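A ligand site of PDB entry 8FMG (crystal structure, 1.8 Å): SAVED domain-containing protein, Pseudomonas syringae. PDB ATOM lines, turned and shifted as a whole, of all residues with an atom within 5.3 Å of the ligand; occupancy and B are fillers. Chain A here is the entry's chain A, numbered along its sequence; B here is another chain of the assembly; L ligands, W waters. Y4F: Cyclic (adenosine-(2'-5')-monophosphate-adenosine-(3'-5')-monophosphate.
Water W4 lies within hydrogen-bond range of O44 of the ligand and O of Tyr 304. Water W1 lies within hydrogen-bond range of OD1 of Asp 365 and O2' of the ligand. Water W3 lies within hydrogen-bond range of N42 of the ligand and N of Ala 343. Water W6 lies within hydrogen-bond range of N1 of the ligand (3.0 Å) and OE1 of Glu 328 of chain B (3.3 Å). Water W5 lies within hydrogen-bond range of OE1 of Glu 328 of chain B (2.8 Å) and N01 of the ligand (3.1 Å). Water W2 bridges O of Ala 339 (2.7 Å) and OD1 of Asp 365 (2.7 Å).
O23 of the ligand sits at hydrogen-bond distance from O of Ile 341 (2.7 Å). NE2 of His 138 is in hydrogen-bond range of O29 of the ligand, at 3.0 Å. A nitrogen (N35) of the ligand lies within hydrogen-bond range of the guanidinium group of Arg 232 of chain B (3.0 Å). The backbone NH (N) of Ala 343 sits at hydrogen-bond distance from an oxygen (O23) of the ligand. O of Asp 231 of chain B is in hydrogen-bond range of N64 of the ligand (3.0 Å). O19 of the ligand is in salt-bridge range of NH1 of Arg 242, at 2.9 Å. The side-chain carboxylate of Asp 231 of chain B lies within hydrogen-bond range of a nitrogen (N64) of the ligand (2.8 Å). O2' of the ligand lies within hydrogen-bond range of N of His 357 of chain B (2.9 Å). N of Gln 356 of chain B sits at hydrogen-bond distance from O30 of the ligand, 2.8 Å away. A nitrogen (N7) of the ligand is in hydrogen-bond range of the guanidinium group (NE) of Arg 366, 3.1 Å away. The side-chain hydroxyl (OG) of Ser 277 is in hydrogen-bond range of an oxygen (O44) of the ligand, at 2.7 Å.
The side-chain carboxylate (OD2) of Asp 231 of chain B lies within salt-bridge range of the guanidinium group (NE) of Arg 242. The backbone carbonyl oxygen (O) of Ala 340 sits at hydrogen-bond distance from the backbone NH (N) of Ser 277 (2.8 Å). A ring nitrogen (NE2) of His 357 of chain B lies within hydrogen-bond range of the side-chain carboxylate (OE1) of Glu 328 of chain B, at 2.8 Å. A ring nitrogen (ND1) of His 138 lies within hydrogen-bond range of the side-chain carboxylate of Asp 218 (3.4 Å). The backbone NH (N) of Ile 341 lies close to the side-chain hydroxyl (OG) of Ser 277 (3.4 Å). N of Tyr 304 sits close to O of Ser 277 (3.5 Å). NE2 of Gln 356 of chain B sits at hydrogen-bond distance from O of Arg 366 (2.9 Å). The side-chain hydroxyl (OG1) of Thr 355 of chain B sits at hydrogen-bond distance from the backbone carbonyl oxygen (O) of His 357 of chain B.
Residues that only touch the ligand: Ala 217, Thr 355 of chain B, Pro 342, Phe 139, Phe 240, Ala 340, Leu 216, Tyr 304, Ala 278, Ile 219, Pro 281, Ala 339, Gln 279 and Phe 374. 24 residues have an atom within 4 Å of the ligand: His 138, Phe 139, Leu 216, Ala 217, Ile 219, Phe 240, Arg 242, Ser 277, Ala 278, Gln 279, Pro 281, Tyr 304, Ala 339, Ala 340, Ile 341, Pro 342, Ala 343, Arg 366, Phe 374, Asp 231 of chain B, Arg 232 of chain B, Thr 355 of chain B, Gln 356 of chain B and His 357 of chain B. The nearest printed residue that does not touch the ligand is Val 280 (4.4 Å).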
ATOM      1  N   HIS A 138     -11.603 -21.034 -13.073  1.00  0.00           N
ATOM      2  CA  HIS A 138     -12.221 -22.350 -13.161  1.00  0.00           C
ATOM      3  C   HIS A 138     -12.608 -22.726 -14.580  1.00  0.00           C
ATOM      4  O   HIS A 138     -13.026 -23.866 -14.804  1.00  0.00           O
ATOM      5  CB  HIS A 138     -13.445 -22.439 -12.235  1.00  0.00           C
ATOM      6  CG  HIS A 138     -14.685 -21.801 -12.771  1.00  0.00           C
ATOM      7  ND1 HIS A 138     -15.001 -20.474 -12.538  1.00  0.00           N
ATOM      8  CD2 HIS A 138     -15.731 -22.321 -13.457  1.00  0.00           C
ATOM      9  CE1 HIS A 138     -16.169 -20.198 -13.096  1.00  0.00           C
ATOM     10  NE2 HIS A 138     -16.636 -21.304 -13.663  1.00  0.00           N
ATOM     11  N   PHE A 139     -12.479 -21.806 -15.535  1.00  0.00           N
ATOM     12  CA  PHE A 139     -12.677 -22.132 -16.941  1.00  0.00           C
ATOM     13  C   PHE A 139     -11.422 -22.805 -17.497  1.00  0.00           C
ATOM     14  O   PHE A 139     -10.328 -22.706 -16.945  1.00  0.00           O
ATOM     15  CB  PHE A 139     -12.995 -20.884 -17.752  1.00  0.00           C
ATOM     16  CG  PHE A 139     -14.136 -20.077 -17.208  1.00  0.00           C
ATOM     17  CD1 PHE A 139     -15.435 -20.438 -17.479  1.00  0.00           C
ATOM     18  CD2 PHE A 139     -13.899 -18.977 -16.417  1.00  0.00           C
ATOM     19  CE1 PHE A 139     -16.484 -19.710 -16.974  1.00  0.00           C
ATOM     20  CE2 PHE A 139     -14.937 -18.241 -15.913  1.00  0.00           C
ATOM     21  CZ  PHE A 139     -16.234 -18.606 -16.193  1.00  0.00           C
ATOM     22  N   ARG A 178     -13.237 -28.706  -8.396  1.00  0.00           N
ATOM     23  CA  ARG A 178     -13.703 -27.696  -7.441  1.00  0.00           C
ATOM     24  C   ARG A 178     -14.137 -28.409  -6.177  1.00  0.00           C
ATOM     25  O   ARG A 178     -15.317 -28.637  -5.910  1.00  0.00           O
ATOM     26  CB  ARG A 178     -14.804 -26.844  -8.053  1.00  0.00           C
ATOM     27  CG  ARG A 178     -14.293 -25.870  -9.105  1.00  0.00           C
ATOM     28  CD  ARG A 178     -15.328 -24.834  -9.451  1.00  0.00           C
ATOM     29  NE  ARG A 178     -16.564 -25.425  -9.944  1.00  0.00           N
ATOM     30  CZ  ARG A 178     -17.654 -24.718 -10.240  1.00  0.00           C
ATOM     31  NH1 ARG A 178     -17.689 -23.411 -10.068  1.00  0.00           N
ATOM     32  NH2 ARG A 178     -18.719 -25.346 -10.731  1.00  0.00           N
ATOM     33  N   LEU A 216     -16.406 -11.944 -12.947  1.00  0.00           N
ATOM     34  CA  LEU A 216     -16.558 -13.044 -13.921  1.00  0.00           C
ATOM     35  C   LEU A 216     -15.892 -14.244 -13.243  1.00  0.00           C
ATOM     36  O   LEU A 216     -14.686 -14.465 -13.383  1.00  0.00           O
ATOM     37  CB  LEU A 216     -15.931 -12.715 -15.253  1.00  0.00           C
ATOM     38  CG  LEU A 216     -16.540 -13.407 -16.481  1.00  0.00           C
ATOM     39  CD1 LEU A 216     -15.929 -12.869 -17.761  1.00  0.00           C
ATOM     40  CD2 LEU A 216     -16.353 -14.900 -16.393  1.00  0.00           C
ATOM     41  N   ALA A 217     -16.698 -14.990 -12.483  1.00  0.00           N
ATOM     42  CA  ALA A 217     -16.177 -16.051 -11.636  1.00  0.00           C
ATOM     43  C   ALA A 217     -17.295 -17.042 -11.357  1.00  0.00           C
ATOM     44  O   ALA A 217     -18.415 -16.888 -11.834  1.00  0.00           O
ATOM     45  CB  ALA A 217     -15.615 -15.481 -10.322  1.00  0.00           C
ATOM     46  N   ASP A 218     -16.975 -18.067 -10.562  1.00  0.00           N
ATOM     47  CA  ASP A 218     -17.969 -19.049 -10.188  1.00  0.00           C
ATOM     48  C   ASP A 218     -19.243 -18.360  -9.718  1.00  0.00           C
ATOM     49  O   ASP A 218     -19.184 -17.414  -8.916  1.00  0.00           O
ATOM     50  CB  ASP A 218     -17.438 -19.959  -9.084  1.00  0.00           C
ATOM     51  CG  ASP A 218     -15.978 -20.324  -9.282  1.00  0.00           C
ATOM     52  OD1 ASP A 218     -15.147 -19.396  -9.345  1.00  0.00           O
ATOM     53  OD2 ASP A 218     -15.668 -21.532  -9.379  1.00  0.00           O
ATOM     54  N   ILE A 219     -20.387 -18.820 -10.216  1.00  0.00           N
ATOM     55  CA  ILE A 219     -21.660 -18.272  -9.742  1.00  0.00           C
ATOM     56  C   ILE A 219     -21.726 -18.251  -8.224  1.00  0.00           C
ATOM     57  O   ILE A 219     -22.043 -17.200  -7.655  1.00  0.00           O
ATOM     58  CB  ILE A 219     -22.835 -19.051 -10.376  1.00  0.00           C
ATOM     59  CG1 ILE A 219     -22.907 -18.739 -11.872  1.00  0.00           C
ATOM     60  CG2 ILE A 219     -24.144 -18.658  -9.700  1.00  0.00           C
ATOM     61  CD1 ILE A 219     -23.898 -19.576 -12.613  1.00  0.00           C
ATOM     62  N   LEU A 222     -19.474 -15.416  -6.926  1.00  0.00           N
ATOM     63  CA  LEU A 222     -20.031 -14.098  -7.172  1.00  0.00           C
ATOM     64  C   LEU A 222     -21.166 -13.804  -6.193  1.00  0.00           C
ATOM     65  O   LEU A 222     -21.344 -12.652  -5.763  1.00  0.00           O
ATOM     66  CB  LEU A 222     -20.527 -13.986  -8.606  1.00  0.00           C
ATOM     67  CG  LEU A 222     -19.418 -13.986  -9.659  1.00  0.00           C
ATOM     68  CD1 LEU A 222     -20.047 -13.910 -11.035  1.00  0.00           C
ATOM     69  CD2 LEU A 222     -18.458 -12.840  -9.448  1.00  0.00           C
ATOM     70  N   PHE A 240     -19.216  -7.613 -17.590  1.00  0.00           N
ATOM     71  CA  PHE A 240     -18.428  -8.063 -18.721  1.00  0.00           C
ATOM     72  C   PHE A 240     -19.355  -8.732 -19.730  1.00  0.00           C
ATOM     73  O   PHE A 240     -20.173  -9.582 -19.368  1.00  0.00           O
ATOM     74  CB  PHE A 240     -17.333  -9.046 -18.287  1.00  0.00           C
ATOM     75  CG  PHE A 240     -16.429  -9.464 -19.410  1.00  0.00           C
ATOM     76  CD1 PHE A 240     -16.793 -10.474 -20.273  1.00  0.00           C
ATOM     77  CD2 PHE A 240     -15.204  -8.832 -19.596  1.00  0.00           C
ATOM     78  CE1 PHE A 240     -15.965 -10.856 -21.315  1.00  0.00           C
ATOM     79  CE2 PHE A 240     -14.379  -9.223 -20.635  1.00  0.00           C
ATOM     80  CZ  PHE A 240     -14.754 -10.229 -21.490  1.00  0.00           C
ATOM     81  N   HIS A 241     -19.231  -8.332 -20.996  1.00  0.00           N
ATOM     82  CA  HIS A 241     -20.133  -8.755 -22.060  1.00  0.00           C
ATOM     83  C   HIS A 241     -19.319  -9.346 -23.204  1.00  0.00           C
ATOM     84  O   HIS A 241     -18.299  -8.775 -23.610  1.00  0.00           O
ATOM     85  CB  HIS A 241     -20.957  -7.560 -22.556  1.00  0.00           C
ATOM     86  CG  HIS A 241     -22.146  -7.929 -23.386  1.00  0.00           C
ATOM     87  ND1 HIS A 241     -22.118  -7.974 -24.758  1.00  0.00           N
ATOM     88  CD2 HIS A 241     -23.413  -8.243 -23.022  1.00  0.00           C
ATOM     89  CE1 HIS A 241     -23.310  -8.321 -25.213  1.00  0.00           C
ATOM     90  NE2 HIS A 241     -24.113  -8.484 -24.181  1.00  0.00           N
ATOM     91  N   ARG A 242     -19.763 -10.491 -23.717  1.00  0.00           N
ATOM     92  CA  ARG A 242     -18.979 -11.172 -24.740  1.00  0.00           C
ATOM     93  C   ARG A 242     -18.731 -10.290 -25.956  1.00  0.00           C
ATOM     94  O   ARG A 242     -17.657 -10.387 -26.567  1.00  0.00           O
ATOM     95  CB  ARG A 242     -19.671 -12.466 -25.159  1.00  0.00           C
ATOM     96  CG  ARG A 242     -19.479 -13.607 -24.196  1.00  0.00           C
ATOM     97  CD  ARG A 242     -20.434 -14.717 -24.541  1.00  0.00           C
ATOM     98  NE  ARG A 242     -20.214 -15.906 -23.717  1.00  0.00           N
ATOM     99  CZ  ARG A 242     -20.709 -16.053 -22.492  1.00  0.00           C
ATOM    100  NH1 ARG A 242     -21.415 -15.085 -21.905  1.00  0.00           N
ATOM    101  NH2 ARG A 242     -20.473 -17.177 -21.836  1.00  0.00           N
ATOM    102  N   SER A 277     -29.711 -16.623 -18.289  1.00  0.00           N
ATOM    103  CA  SER A 277     -28.734 -16.847 -19.348  1.00  0.00           C
ATOM    104  C   SER A 277     -29.169 -17.965 -20.278  1.00  0.00           C
ATOM    105  O   SER A 277     -28.782 -17.992 -21.449  1.00  0.00           O
ATOM    106  CB  SER A 277     -27.384 -17.219 -18.739  1.00  0.00           C
ATOM    107  OG  SER A 277     -26.904 -16.203 -17.880  1.00  0.00           O
ATOM    108  N   ALA A 278     -29.936 -18.906 -19.748  1.00  0.00           N
ATOM    109  CA  ALA A 278     -30.320 -20.097 -20.494  1.00  0.00           C
ATOM    110  C   ALA A 278     -31.472 -20.737 -19.742  1.00  0.00           C
ATOM    111  O   ALA A 278     -31.767 -20.370 -18.598  1.00  0.00           O
ATOM    112  CB  ALA A 278     -29.140 -21.045 -20.664  1.00  0.00           C
ATOM    113  N   GLN A 279     -32.117 -21.693 -20.393  1.00  0.00           N
ATOM    114  CA  GLN A 279     -33.169 -22.474 -19.751  1.00  0.00           C
ATOM    115  C   GLN A 279     -32.531 -23.601 -18.954  1.00  0.00           C
ATOM    116  O   GLN A 279     -31.858 -24.468 -19.524  1.00  0.00           O
ATOM    117  CB  GLN A 279     -34.138 -23.032 -20.781  1.00  0.00           C
ATOM    118  CG  GLN A 279     -35.262 -23.891 -20.185  1.00  0.00           C
ATOM    119  CD  GLN A 279     -36.152 -23.114 -19.231  1.00  0.00           C
ATOM    120  OE1 GLN A 279     -36.627 -22.028 -19.553  1.00  0.00           O
ATOM    121  NE2 GLN A 279     -36.380 -23.675 -18.049  1.00  0.00           N
ATOM    122  N   VAL A 280     -32.727 -23.595 -17.640  1.00  0.00           N
ATOM    123  CA  VAL A 280     -32.233 -24.664 -16.773  1.00  0.00           C
ATOM    124  C   VAL A 280     -33.201 -25.832 -16.876  1.00  0.00           C
ATOM    125  O   VAL A 280     -34.367 -25.692 -16.465  1.00  0.00           O
ATOM    126  CB  VAL A 280     -32.098 -24.174 -15.316  1.00  0.00           C
ATOM    127  CG1 VAL A 280     -31.771 -25.333 -14.408  1.00  0.00           C
ATOM    128  CG2 VAL A 280     -31.019 -23.108 -15.215  1.00  0.00           C
ATOM    129  N   PRO A 281     -32.798 -26.980 -17.422  1.00  0.00           N
ATOM    130  CA  PRO A 281     -33.746 -28.104 -17.541  1.00  0.00           C
ATOM    131  C   PRO A 281     -34.119 -28.623 -16.160  1.00  0.00           C
ATOM    132  O   PRO A 281     -33.258 -28.992 -15.365  1.00  0.00           O
ATOM    133  CB  PRO A 281     -32.958 -29.150 -18.344  1.00  0.00           C
ATOM    134  CG  PRO A 281     -31.801 -28.397 -18.967  1.00  0.00           C
ATOM    135  CD  PRO A 281     -31.471 -27.294 -17.996  1.00  0.00           C
ATOM    136  N   TYR A 304     -27.242 -15.382 -23.143  1.00  0.00           N
ATOM    137  CA  TYR A 304     -26.036 -14.902 -22.500  1.00  0.00           C
ATOM    138  C   TYR A 304     -25.865 -13.392 -22.650  1.00  0.00           C
ATOM    139  O   TYR A 304     -25.070 -12.795 -21.910  1.00  0.00           O
ATOM    140  CB  TYR A 304     -24.783 -15.551 -23.078  1.00  0.00           C
ATOM    141  CG  TYR A 304     -24.555 -16.991 -22.741  1.00  0.00           C
ATOM    142  CD1 TYR A 304     -25.414 -17.698 -21.908  1.00  0.00           C
ATOM    143  CD2 TYR A 304     -23.454 -17.657 -23.252  1.00  0.00           C
ATOM    144  CE1 TYR A 304     -25.182 -19.022 -21.608  1.00  0.00           C
ATOM    145  CE2 TYR A 304     -23.219 -18.976 -22.965  1.00  0.00           C
ATOM    146  CZ  TYR A 304     -24.082 -19.654 -22.144  1.00  0.00           C
ATOM    147  OH  TYR A 304     -23.825 -20.979 -21.861  1.00  0.00           O
ATOM    148  N   ALA A 339     -28.968 -21.884 -10.850  1.00  0.00           N
ATOM    149  CA  ALA A 339     -28.926 -20.605 -11.543  1.00  0.00           C
ATOM    150  C   ALA A 339     -28.108 -20.691 -12.820  1.00  0.00           C
ATOM    151  O   ALA A 339     -26.936 -21.088 -12.783  1.00  0.00           O
ATOM    152  CB  ALA A 339     -28.359 -19.518 -10.620  1.00  0.00           C
ATOM    153  N   ALA A 340     -28.719 -20.323 -13.932  1.00  0.00           N
ATOM    154  CA  ALA A 340     -28.013 -20.020 -15.173  1.00  0.00           C
ATOM    155  C   ALA A 340     -28.224 -18.522 -15.377  1.00  0.00           C
ATOM    156  O   ALA A 340     -29.206 -18.099 -15.985  1.00  0.00           O
ATOM    157  CB  ALA A 340     -28.527 -20.831 -16.344  1.00  0.00           C
ATOM    158  N   ILE A 341     -27.315 -17.720 -14.834  1.00  0.00           N
ATOM    159  CA  ILE A 341     -27.470 -16.259 -14.815  1.00  0.00           C
ATOM    160  C   ILE A 341     -26.144 -15.610 -15.154  1.00  0.00           C
ATOM    161  O   ILE A 341     -25.070 -16.143 -14.868  1.00  0.00           O
ATOM    162  CB  ILE A 341     -27.955 -15.753 -13.444  1.00  0.00           C
ATOM    163  CG1 ILE A 341     -26.960 -16.148 -12.351  1.00  0.00           C
ATOM    164  CG2 ILE A 341     -29.335 -16.312 -13.130  1.00  0.00           C
ATOM    165  CD1 ILE A 341     -27.282 -15.544 -11.002  1.00  0.00           C
ATOM    166  N   PRO A 342     -26.198 -14.416 -15.752  1.00  0.00           N
ATOM    167  CA  PRO A 342     -24.965 -13.667 -15.996  1.00  0.00           C
ATOM    168  C   PRO A 342     -24.302 -13.224 -14.699  1.00  0.00           C
ATOM    169  O   PRO A 342     -24.941 -13.058 -13.653  1.00  0.00           O
ATOM    170  CB  PRO A 342     -25.431 -12.457 -16.819  1.00  0.00           C
ATOM    171  CG  PRO A 342     -26.742 -12.888 -17.425  1.00  0.00           C
ATOM    172  CD  PRO A 342     -27.376 -13.768 -16.369  1.00  0.00           C
ATOM    173  N   ALA A 343     -22.994 -12.994 -14.800  1.00  0.00           N
ATOM    174  CA  ALA A 343     -22.162 -12.755 -13.628  1.00  0.00           C
ATOM    175  C   ALA A 343     -22.634 -11.568 -12.815  1.00  0.00           C
ATOM    176  O   ALA A 343     -22.653 -11.618 -11.577  1.00  0.00           O
ATOM    177  CB  ALA A 343     -20.715 -12.556 -14.076  1.00  0.00           C
ATOM    178  N   ALA A 346     -25.507 -12.494 -10.595  1.00  0.00           N
ATOM    179  CA  ALA A 346     -25.094 -13.301  -9.457  1.00  0.00           C
ATOM    180  C   ALA A 346     -24.607 -12.417  -8.310  1.00  0.00           C
ATOM    181  O   ALA A 346     -24.916 -12.669  -7.139  1.00  0.00           O
ATOM    182  CB  ALA A 346     -23.994 -14.283  -9.880  1.00  0.00           C
ATOM    183  N   ASP A 365     -24.279 -25.901  -8.460  1.00  0.00           N
ATOM    184  CA  ASP A 365     -23.593 -25.463  -9.674  1.00  0.00           C
ATOM    185  C   ASP A 365     -23.249 -26.694 -10.502  1.00  0.00           C
ATOM    186  O   ASP A 365     -23.166 -27.816  -9.985  1.00  0.00           O
ATOM    187  CB  ASP A 365     -22.340 -24.645  -9.350  1.00  0.00           C
ATOM    188  CG  ASP A 365     -21.880 -23.778 -10.509  1.00  0.00           C
ATOM    189  OD1 ASP A 365     -22.665 -23.599 -11.474  1.00  0.00           O
ATOM    190  OD2 ASP A 365     -20.736 -23.273 -10.469  1.00  0.00           O
ATOM    191  N   ARG A 366     -23.040 -26.474 -11.788  1.00  0.00           N
ATOM    192  CA  ARG A 366     -22.667 -27.556 -12.696  1.00  0.00           C
ATOM    193  C   ARG A 366     -21.297 -28.120 -12.322  1.00  0.00           C
ATOM    194  O   ARG A 366     -20.369 -27.369 -12.017  1.00  0.00           O
ATOM    195  CB  ARG A 366     -22.656 -27.055 -14.135  1.00  0.00           C
ATOM    196  CG  ARG A 366     -24.008 -26.589 -14.642  1.00  0.00           C
ATOM    197  CD  ARG A 366     -24.937 -27.763 -14.824  1.00  0.00           C
ATOM    198  NE  ARG A 366     -26.203 -27.377 -15.435  1.00  0.00           N
ATOM    199  CZ  ARG A 366     -27.137 -28.232 -15.817  1.00  0.00           C
ATOM    200  NH1 ARG A 366     -26.940 -29.539 -15.750  1.00  0.00           N
ATOM    201  NH2 ARG A 366     -28.293 -27.769 -16.275  1.00  0.00           N
ATOM    202  N   PHE A 374     -25.805 -31.003 -11.546  1.00  0.00           N
ATOM    203  CA  PHE A 374     -25.779 -30.006 -10.486  1.00  0.00           C
ATOM    204  C   PHE A 374     -25.278 -30.656  -9.199  1.00  0.00           C
ATOM    205  O   PHE A 374     -25.683 -31.763  -8.842  1.00  0.00           O
ATOM    206  CB  PHE A 374     -27.170 -29.419 -10.236  1.00  0.00           C
ATOM    207  CG  PHE A 374     -27.567 -28.359 -11.214  1.00  0.00           C
ATOM    208  CD1 PHE A 374     -26.967 -27.104 -11.213  1.00  0.00           C
ATOM    209  CD2 PHE A 374     -28.574 -28.603 -12.129  1.00  0.00           C
ATOM    210  CE1 PHE A 374     -27.350 -26.129 -12.120  1.00  0.00           C
ATOM    211  CE2 PHE A 374     -28.969 -27.636 -13.035  1.00  0.00           C
ATOM    212  CZ  PHE A 374     -28.363 -26.401 -13.025  1.00  0.00           C
ATOM    213  N   ASP B 231     -14.057 -16.954 -24.713  1.00  0.00           N
ATOM    214  CA  ASP B 231     -14.736 -15.709 -25.050  1.00  0.00           C
ATOM    215  C   ASP B 231     -14.824 -14.777 -23.852  1.00  0.00           C
ATOM    216  O   ASP B 231     -15.725 -13.940 -23.783  1.00  0.00           O
ATOM    217  CB  ASP B 231     -16.139 -16.002 -25.632  1.00  0.00           C
ATOM    218  CG  ASP B 231     -17.035 -16.831 -24.711  1.00  0.00           C
ATOM    219  OD1 ASP B 231     -16.657 -17.049 -23.539  1.00  0.00           O
ATOM    220  OD2 ASP B 231     -18.116 -17.263 -25.154  1.00  0.00           O
ATOM    221  N   ARG B 232     -13.877 -14.884 -22.921  1.00  0.00           N
ATOM    222  CA  ARG B 232     -13.885 -14.128 -21.678  1.00  0.00           C
ATOM    223  C   ARG B 232     -12.571 -13.381 -21.478  1.00  0.00           C
ATOM    224  O   ARG B 232     -11.997 -13.355 -20.384  1.00  0.00           O
ATOM    225  CB  ARG B 232     -14.191 -15.041 -20.493  1.00  0.00           C
ATOM    226  CG  ARG B 232     -13.372 -16.326 -20.466  1.00  0.00           C
ATOM    227  CD  ARG B 232     -13.913 -17.335 -19.438  1.00  0.00           C
ATOM    228  NE  ARG B 232     -15.285 -17.745 -19.735  1.00  0.00           N
ATOM    229  CZ  ARG B 232     -15.615 -18.626 -20.667  1.00  0.00           C
ATOM    230  NH1 ARG B 232     -14.708 -19.220 -21.419  1.00  0.00           N
ATOM    231  NH2 ARG B 232     -16.909 -18.896 -20.866  1.00  0.00           N
ATOM    232  N   GLU B 328     -31.206 -27.980 -25.904  1.00  0.00           N
ATOM    233  CA  GLU B 328     -30.795 -28.727 -24.726  1.00  0.00           C
ATOM    234  C   GLU B 328     -31.948 -28.887 -23.746  1.00  0.00           C
ATOM    235  O   GLU B 328     -32.023 -29.898 -23.028  1.00  0.00           O
ATOM    236  CB  GLU B 328     -29.598 -28.040 -24.060  1.00  0.00           C
ATOM    237  CG  GLU B 328     -28.385 -27.946 -24.979  1.00  0.00           C
ATOM    238  CD  GLU B 328     -27.166 -27.329 -24.313  1.00  0.00           C
ATOM    239  OE1 GLU B 328     -27.220 -27.053 -23.097  1.00  0.00           O
ATOM    240  OE2 GLU B 328     -26.156 -27.131 -25.016  1.00  0.00           O
ATOM    241  N   THR B 355     -18.204 -22.608 -21.216  1.00  0.00           N
ATOM    242  CA  THR B 355     -18.691 -22.393 -19.866  1.00  0.00           C
ATOM    243  C   THR B 355     -18.403 -23.616 -19.005  1.00  0.00           C
ATOM    244  O   THR B 355     -18.001 -24.678 -19.498  1.00  0.00           O
ATOM    245  CB  THR B 355     -20.199 -22.100 -19.855  1.00  0.00           C
ATOM    246  OG1 THR B 355     -20.878 -23.144 -20.585  1.00  0.00           O
ATOM    247  CG2 THR B 355     -20.509 -20.746 -20.468  1.00  0.00           C
ATOM    248  N   GLN B 356     -18.611 -23.477 -17.694  1.00  0.00           N
ATOM    249  CA  GLN B 356     -18.587 -24.649 -16.825  1.00  0.00           C
ATOM    250  C   GLN B 356     -19.631 -25.667 -17.268  1.00  0.00           C
ATOM    251  O   GLN B 356     -19.362 -26.879 -17.284  1.00  0.00           O
ATOM    252  CB  GLN B 356     -18.810 -24.214 -15.376  1.00  0.00           C
ATOM    253  CG  GLN B 356     -18.949 -25.351 -14.365  1.00  0.00           C
ATOM    254  CD  GLN B 356     -17.625 -25.968 -13.954  1.00  0.00           C
ATOM    255  OE1 GLN B 356     -16.556 -25.536 -14.381  1.00  0.00           O
ATOM    256  NE2 GLN B 356     -17.699 -27.000 -13.118  1.00  0.00           N
ATOM    257  N   HIS B 357     -20.818 -25.196 -17.637  1.00  0.00           N
ATOM    258  CA  HIS B 357     -21.841 -26.085 -18.187  1.00  0.00           C
ATOM    259  C   HIS B 357     -21.397 -26.663 -19.513  1.00  0.00           C
ATOM    260  O   HIS B 357     -20.937 -25.931 -20.396  1.00  0.00           O
ATOM    261  CB  HIS B 357     -23.157 -25.331 -18.378  1.00  0.00           C
ATOM    262  CG  HIS B 357     -24.108 -26.008 -19.333  1.00  0.00           C
ATOM    263  ND1 HIS B 357     -24.782 -27.168 -19.013  1.00  0.00           N
ATOM    264  CD2 HIS B 357     -24.483 -25.682 -20.593  1.00  0.00           C
ATOM    265  CE1 HIS B 357     -25.539 -27.520 -20.036  1.00  0.00           C
ATOM    266  NE2 HIS B 357     -25.381 -26.647 -21.011  1.00  0.00           N
HETATM  267  C4  Y4F L   1     -25.781 -22.978 -17.498  1.00  0.00           C
HETATM  268  C8  Y4F L   1     -25.882 -23.614 -15.403  1.00  0.00           C
HETATM  269  C1' Y4F L   1     -24.264 -21.729 -15.943  1.00  0.00           C
HETATM  270  C16 Y4F L   1     -24.104 -19.049 -17.939  1.00  0.00           C
HETATM  271  C2  Y4F L   1     -26.152 -22.844 -19.666  1.00  0.00           C
HETATM  272  C2' Y4F L   1     -22.984 -21.815 -16.808  1.00  0.00           C
HETATM  273  C21 Y4F L   1     -21.506 -16.810 -16.339  1.00  0.00           C
HETATM  274  C22 Y4F L   1     -21.685 -16.935 -14.814  1.00  0.00           C
HETATM  275  C24 Y4F L   1     -20.233 -16.905 -14.321  1.00  0.00           C
HETATM  276  C25 Y4F L   1     -19.562 -18.252 -14.229  1.00  0.00           C
HETATM  277  C3' Y4F L   1     -22.397 -20.427 -16.634  1.00  0.00           C
HETATM  278  C32 Y4F L   1     -20.388 -15.784 -16.380  1.00  0.00           C
HETATM  279  C34 Y4F L   1     -18.949 -16.992 -18.097  1.00  0.00           C
HETATM  280  C36 Y4F L   1     -19.376 -14.883 -18.542  1.00  0.00           C
HETATM  281  C37 Y4F L   1     -18.592 -15.445 -19.539  1.00  0.00           C
HETATM  282  C38 Y4F L   1     -18.205 -14.672 -20.617  1.00  0.00           C
HETATM  283  C4' Y4F L   1     -23.653 -19.590 -16.597  1.00  0.00           C
HETATM  284  C40 Y4F L   1     -19.340 -12.843 -19.709  1.00  0.00           C
HETATM  285  C5  Y4F L   1     -26.684 -24.001 -17.354  1.00  0.00           C
HETATM  286  C6  Y4F L   1     -27.352 -24.454 -18.505  1.00  0.00           C
HETATM  287  N01 Y4F L   1     -28.247 -25.437 -18.508  1.00  0.00           N
HETATM  288  N1  Y4F L   1     -27.057 -23.838 -19.677  1.00  0.00           N
HETATM  289  N3  Y4F L   1     -25.469 -22.344 -18.641  1.00  0.00           N
HETATM  290  N33 Y4F L   1     -19.601 -15.880 -17.615  1.00  0.00           N
HETATM  291  N35 Y4F L   1     -18.343 -16.780 -19.231  1.00  0.00           N
HETATM  292  N39 Y4F L   1     -18.588 -13.355 -20.677  1.00  0.00           N
HETATM  293  N42 Y4F L   1     -19.744 -13.578 -18.627  1.00  0.00           N
HETATM  294  N64 Y4F L   1     -17.464 -15.144 -21.604  1.00  0.00           N
HETATM  295  N7  Y4F L   1     -26.743 -24.397 -16.011  1.00  0.00           N
HETATM  296  N9  Y4F L   1     -25.282 -22.718 -16.263  1.00  0.00           N
HETATM  297  O17 Y4F L   1     -23.042 -18.320 -18.568  1.00  0.00           O
HETATM  298  O19 Y4F L   1     -21.874 -16.256 -19.298  1.00  0.00           O
HETATM  299  O2' Y4F L   1     -22.224 -22.928 -16.391  1.00  0.00           O
HETATM  300  O20 Y4F L   1     -22.762 -16.404 -16.891  1.00  0.00           O
HETATM  301  O23 Y4F L   1     -22.421 -15.831 -14.288  1.00  0.00           O
HETATM  302  O26 Y4F L   1     -19.627 -18.920 -15.511  1.00  0.00           O
HETATM  303  O28 Y4F L   1     -21.669 -20.421 -15.417  1.00  0.00           O
HETATM  304  O29 Y4F L   1     -19.587 -21.124 -14.272  1.00  0.00           O
HETATM  305  O30 Y4F L   1     -19.578 -20.998 -16.874  1.00  0.00           O
HETATM  306  O31 Y4F L   1     -19.522 -16.091 -15.303  1.00  0.00           O
HETATM  307  O4' Y4F L   1     -24.746 -20.422 -16.117  1.00  0.00           O
HETATM  308  O44 Y4F L   1     -24.389 -16.183 -18.784  1.00  0.00           O
HETATM  309  P18 Y4F L   1     -23.016 -16.717 -18.444  1.00  0.00           P
HETATM  310  P27 Y4F L   1     -20.059 -20.465 -15.546  1.00  0.00           P
HETATM  311  O   HOH W   1     -21.647 -23.214 -13.814  1.00  0.00           O
HETATM  312  O   HOH W   2     -25.277 -23.161 -12.185  1.00  0.00           O
HETATM  313  O   HOH W   3     -22.225 -12.462 -17.588  1.00  0.00           O
HETATM  314  O   HOH W   4     -24.043 -13.681 -19.385  1.00  0.00           O
HETATM  315  O   HOH W   5     -29.077 -26.986 -21.033  1.00  0.00           O
HETATM  316  O   HOH W   6     -28.083 -23.945 -22.544  1.00  0.00           O
